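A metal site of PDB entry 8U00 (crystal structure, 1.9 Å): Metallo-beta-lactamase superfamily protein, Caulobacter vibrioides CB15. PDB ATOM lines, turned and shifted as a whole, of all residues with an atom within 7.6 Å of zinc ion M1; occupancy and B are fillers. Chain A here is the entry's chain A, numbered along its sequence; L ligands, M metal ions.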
ATOM      1  N   TRP A  10     -11.232 -31.246 -17.529  1.00  0.00           N
ATOM      2  CA  TRP A  10     -12.488 -30.511 -17.727  1.00  0.00           C
ATOM      3  C   TRP A  10     -13.095 -30.040 -16.415  1.00  0.00           C
ATOM      4  O   TRP A  10     -13.854 -29.069 -16.406  1.00  0.00           O
ATOM      5  CB  TRP A  10     -13.529 -31.374 -18.441  1.00  0.00           C
ATOM      6  CG  TRP A  10     -13.341 -31.597 -19.903  1.00  0.00           C
ATOM      7  CD1 TRP A  10     -12.252 -31.259 -20.652  1.00  0.00           C
ATOM      8  CD2 TRP A  10     -14.285 -32.212 -20.792  1.00  0.00           C
ATOM      9  NE1 TRP A  10     -12.450 -31.642 -21.964  1.00  0.00           N
ATOM     10  CE2 TRP A  10     -13.691 -32.225 -22.079  1.00  0.00           C
ATOM     11  CE3 TRP A  10     -15.563 -32.757 -20.630  1.00  0.00           C
ATOM     12  CZ2 TRP A  10     -14.343 -32.768 -23.200  1.00  0.00           C
ATOM     13  CZ3 TRP A  10     -16.216 -33.309 -21.751  1.00  0.00           C
ATOM     14  CH2 TRP A  10     -15.593 -33.307 -23.015  1.00  0.00           C
ATOM     15  N   GLY A  30      -9.487 -27.186 -18.317  1.00  0.00           N
ATOM     16  CA  GLY A  30      -9.772 -27.586 -19.681  1.00  0.00           C
ATOM     17  C   GLY A  30     -10.958 -26.967 -20.392  1.00  0.00           C
ATOM     18  O   GLY A  30     -10.975 -26.973 -21.628  1.00  0.00           O
ATOM     19  N   ILE A  31     -11.971 -26.477 -19.687  1.00  0.00           N
ATOM     20  CA  ILE A  31     -13.189 -25.963 -20.297  1.00  0.00           C
ATOM     21  C   ILE A  31     -13.295 -24.466 -19.995  1.00  0.00           C
ATOM     22  O   ILE A  31     -13.277 -24.065 -18.832  1.00  0.00           O
ATOM     23  CB  ILE A  31     -14.453 -26.680 -19.804  1.00  0.00           C
ATOM     24  CG1 ILE A  31     -14.417 -28.177 -20.178  1.00  0.00           C
ATOM     25  CG2 ILE A  31     -15.672 -26.075 -20.448  1.00  0.00           C
ATOM     26  CD1 ILE A  31     -14.470 -28.402 -21.675  1.00  0.00           C
ATOM     27  N   THR A  77     -21.597 -21.034 -26.243  1.00  0.00           N
ATOM     28  CA  THR A  77     -21.097 -21.417 -27.573  1.00  0.00           C
ATOM     29  C   THR A  77     -21.992 -22.494 -28.188  1.00  0.00           C
ATOM     30  O   THR A  77     -22.716 -22.244 -29.153  1.00  0.00           O
ATOM     31  CB  THR A  77     -19.627 -21.853 -27.525  1.00  0.00           C
ATOM     32  OG1 THR A  77     -19.402 -22.762 -26.452  1.00  0.00           O
ATOM     33  CG2 THR A  77     -18.717 -20.588 -27.278  1.00  0.00           C
ATOM     34  N   HIS A  78     -21.983 -23.707 -27.624  1.00  0.00           N
ATOM     35  CA  HIS A  78     -22.986 -24.684 -28.035  1.00  0.00           C
ATOM     36  C   HIS A  78     -23.494 -25.435 -26.823  1.00  0.00           C
ATOM     37  O   HIS A  78     -22.828 -25.513 -25.771  1.00  0.00           O
ATOM     38  CB  HIS A  78     -22.484 -25.603 -29.186  1.00  0.00           C
ATOM     39  CG  HIS A  78     -21.686 -26.800 -28.748  1.00  0.00           C
ATOM     40  ND1 HIS A  78     -20.358 -26.725 -28.382  1.00  0.00           N
ATOM     41  CD2 HIS A  78     -22.005 -28.126 -28.704  1.00  0.00           C
ATOM     42  CE1 HIS A  78     -19.906 -27.929 -28.096  1.00  0.00           C
ATOM     43  NE2 HIS A  78     -20.886 -28.797 -28.275  1.00  0.00           N
ATOM     44  N   HIS A  80     -24.262 -28.301 -25.634  1.00  0.00           N
ATOM     45  CA  HIS A  80     -24.014 -29.633 -25.081  1.00  0.00           C
ATOM     46  C   HIS A  80     -23.442 -29.511 -23.675  1.00  0.00           C
ATOM     47  O   HIS A  80     -23.060 -28.424 -23.238  1.00  0.00           O
ATOM     48  CB  HIS A  80     -23.079 -30.416 -25.980  1.00  0.00           C
ATOM     49  CG  HIS A  80     -23.739 -30.927 -27.215  1.00  0.00           C
ATOM     50  ND1 HIS A  80     -23.031 -31.241 -28.355  1.00  0.00           N
ATOM     51  CD2 HIS A  80     -25.036 -31.179 -27.500  1.00  0.00           C
ATOM     52  CE1 HIS A  80     -23.855 -31.704 -29.271  1.00  0.00           C
ATOM     53  NE2 HIS A  80     -25.078 -31.658 -28.796  1.00  0.00           N
ATOM     54  N   TYR A  81     -23.401 -30.636 -22.957  1.00  0.00           N
ATOM     55  CA  TYR A  81     -23.158 -30.553 -21.517  1.00  0.00           C
ATOM     56  C   TYR A  81     -21.780 -29.970 -21.221  1.00  0.00           C
ATOM     57  O   TYR A  81     -21.628 -29.227 -20.240  1.00  0.00           O
ATOM     58  CB  TYR A  81     -23.333 -31.927 -20.854  1.00  0.00           C
ATOM     59  CG  TYR A  81     -22.141 -32.847 -20.962  1.00  0.00           C
ATOM     60  CD1 TYR A  81     -21.094 -32.784 -20.041  1.00  0.00           C
ATOM     61  CD2 TYR A  81     -22.067 -33.808 -21.974  1.00  0.00           C
ATOM     62  CE1 TYR A  81     -19.996 -33.648 -20.145  1.00  0.00           C
ATOM     63  CE2 TYR A  81     -20.990 -34.669 -22.071  1.00  0.00           C
ATOM     64  CZ  TYR A  81     -19.958 -34.583 -21.163  1.00  0.00           C
ATOM     65  OH  TYR A  81     -18.878 -35.434 -21.270  1.00  0.00           O
ATOM     66  N   ASP A  82     -20.765 -30.249 -22.053  1.00  0.00           N
ATOM     67  CA  ASP A  82     -19.421 -29.872 -21.613  1.00  0.00           C
ATOM     68  C   ASP A  82     -19.241 -28.351 -21.553  1.00  0.00           C
ATOM     69  O   ASP A  82     -18.383 -27.895 -20.803  1.00  0.00           O
ATOM     70  CB  ASP A  82     -18.311 -30.491 -22.482  1.00  0.00           C
ATOM     71  CG  ASP A  82     -18.398 -30.154 -23.982  1.00  0.00           C
ATOM     72  OD1 ASP A  82     -19.484 -29.914 -24.534  1.00  0.00           O
ATOM     73  OD2 ASP A  82     -17.327 -30.228 -24.630  1.00  0.00           O
ATOM     74  N   HIS A  83     -20.055 -27.589 -22.273  1.00  0.00           N
ATOM     75  CA  HIS A  83     -20.022 -26.125 -22.182  1.00  0.00           C
ATOM     76  C   HIS A  83     -21.243 -25.511 -21.532  1.00  0.00           C
ATOM     77  O   HIS A  83     -21.150 -24.408 -20.996  1.00  0.00           O
ATOM     78  CB  HIS A  83     -19.878 -25.531 -23.585  1.00  0.00           C
ATOM     79  CG  HIS A  83     -18.683 -26.030 -24.283  1.00  0.00           C
ATOM     80  ND1 HIS A  83     -17.408 -25.683 -23.893  1.00  0.00           N
ATOM     81  CD2 HIS A  83     -18.548 -26.960 -25.256  1.00  0.00           C
ATOM     82  CE1 HIS A  83     -16.529 -26.345 -24.632  1.00  0.00           C
ATOM     83  NE2 HIS A  83     -17.205 -27.094 -25.478  1.00  0.00           N
ATOM     84  N   HIS A 154     -21.779 -28.601 -35.968  1.00  0.00           N
ATOM     85  CA  HIS A 154     -21.812 -29.570 -34.881  1.00  0.00           C
ATOM     86  C   HIS A 154     -23.193 -29.649 -34.233  1.00  0.00           C
ATOM     87  O   HIS A 154     -23.694 -30.742 -33.959  1.00  0.00           O
ATOM     88  CB  HIS A 154     -20.741 -29.196 -33.864  1.00  0.00           C
ATOM     89  CG  HIS A 154     -20.646 -30.144 -32.718  1.00  0.00           C
ATOM     90  ND1 HIS A 154     -20.560 -31.516 -32.886  1.00  0.00           N
ATOM     91  CD2 HIS A 154     -20.609 -29.917 -31.385  1.00  0.00           C
ATOM     92  CE1 HIS A 154     -20.473 -32.088 -31.702  1.00  0.00           C
ATOM     93  NE2 HIS A 154     -20.498 -31.156 -30.774  1.00  0.00           N
ATOM     94  N   SER A 179     -16.682 -24.645 -30.856  1.00  0.00           N
ATOM     95  CA  SER A 179     -15.611 -25.636 -30.850  1.00  0.00           C
ATOM     96  C   SER A 179     -15.314 -26.240 -32.213  1.00  0.00           C
ATOM     97  O   SER A 179     -14.285 -26.921 -32.353  1.00  0.00           O
ATOM     98  CB  SER A 179     -15.922 -26.784 -29.869  1.00  0.00           C
ATOM     99  OG  SER A 179     -16.019 -26.313 -28.543  1.00  0.00           O
ATOM    100  N   SER A 181     -16.472 -28.759 -33.540  1.00  0.00           N
ATOM    101  CA  SER A 181     -16.336 -30.196 -33.304  1.00  0.00           C
ATOM    102  C   SER A 181     -17.065 -31.030 -34.356  1.00  0.00           C
ATOM    103  O   SER A 181     -18.049 -30.594 -34.970  1.00  0.00           O
ATOM    104  CB  SER A 181     -16.876 -30.536 -31.927  1.00  0.00           C
ATOM    105  OG  SER A 181     -16.821 -31.920 -31.643  1.00  0.00           O
ATOM    106  N   ALA A 218     -13.176 -22.438 -26.725  1.00  0.00           N
ATOM    107  CA  ALA A 218     -13.939 -23.068 -25.666  1.00  0.00           C
ATOM    108  C   ALA A 218     -13.212 -24.243 -25.006  1.00  0.00           C
ATOM    109  O   ALA A 218     -13.607 -24.647 -23.909  1.00  0.00           O
ATOM    110  CB  ALA A 218     -15.302 -23.544 -26.216  1.00  0.00           C
ATOM    111  N   HIS A 219     -12.157 -24.769 -25.623  1.00  0.00           N
ATOM    112  CA  HIS A 219     -11.293 -25.783 -25.019  1.00  0.00           C
ATOM    113  C   HIS A 219      -9.866 -25.250 -24.895  1.00  0.00           C
ATOM    114  O   HIS A 219      -9.360 -24.629 -25.820  1.00  0.00           O
ATOM    115  CB  HIS A 219     -11.274 -27.058 -25.856  1.00  0.00           C
ATOM    116  CG  HIS A 219     -12.447 -27.953 -25.607  1.00  0.00           C
ATOM    117  ND1 HIS A 219     -12.452 -28.887 -24.598  1.00  0.00           N
ATOM    118  CD2 HIS A 219     -13.648 -28.050 -26.227  1.00  0.00           C
ATOM    119  CE1 HIS A 219     -13.597 -29.535 -24.606  1.00  0.00           C
ATOM    120  NE2 HIS A 219     -14.344 -29.049 -25.581  1.00  0.00           N
ATOM    121  N   GLU A 221      -6.896 -26.635 -25.060  1.00  0.00           N
ATOM    122  CA  GLU A 221      -5.899 -27.044 -26.043  1.00  0.00           C
ATOM    123  C   GLU A 221      -6.118 -26.361 -27.391  1.00  0.00           C
ATOM    124  O   GLU A 221      -5.176 -26.305 -28.204  1.00  0.00           O
ATOM    125  CB  GLU A 221      -5.913 -28.572 -26.190  1.00  0.00           C
ATOM    126  CG  GLU A 221      -7.231 -29.166 -26.690  1.00  0.00           C
ATOM    127  CD  GLU A 221      -8.199 -29.551 -25.578  1.00  0.00           C
ATOM    128  OE1 GLU A 221      -8.033 -29.072 -24.425  1.00  0.00           O
ATOM    129  OE2 GLU A 221      -9.123 -30.358 -25.861  1.00  0.00           O
ATOM    130  N   GLN A 222      -7.314 -25.839 -27.665  1.00  0.00           N
ATOM    131  CA  GLN A 222      -7.515 -25.158 -28.929  1.00  0.00           C
ATOM    132  C   GLN A 222      -6.843 -23.787 -28.964  1.00  0.00           C
ATOM    133  O   GLN A 222      -6.680 -23.233 -30.059  1.00  0.00           O
ATOM    134  CB  GLN A 222      -9.005 -25.014 -29.215  1.00  0.00           C
ATOM    135  CG  GLN A 222      -9.704 -26.343 -29.500  1.00  0.00           C
ATOM    136  CD  GLN A 222     -11.218 -26.214 -29.646  1.00  0.00           C
ATOM    137  OE1 GLN A 222     -11.844 -25.391 -28.986  1.00  0.00           O
ATOM    138  NE2 GLN A 222     -11.815 -27.068 -30.507  1.00  0.00           N
HETATM  139 CL1  LIG L   1     -16.854 -29.742 -28.236  1.00  0.00          CL
HETATM  140 ZN    ZN M   1     -16.487 -29.086 -26.068  1.00  0.00          ZN
HETATM  141 ZN    ZN M   2     -20.833 -31.015 -28.573  1.00  0.00          ZN
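Ser 179 touches zinc ion M1.
Of the 16 residues printed, 4 come within 4 Å of zinc ion M1.
Along chain A the residues within 4 Å of zinc ion M1 span positions 82 to 219.
A ring nitrogen (NE2) of His 83 sits close to the side-chain hydroxyl of Ser 179, at 3.4 Å.
The backbone NH (N) of His 219 lies within hydrogen-bond range of the side-chain amide oxygen (OE1) of Gln 222.
The backbone carbonyl oxygen of Ser 179 lies within hydrogen-bond range of the side-chain amide nitrogen of Gln 222, 3.1 Å away.
Zinc ion M1 is bound by OD2 of Asp 82, NE2 of His 83, NE2 of His 219 and CL1 of the ligand.
Zinc ion M1 has four donor atoms within binding distance.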
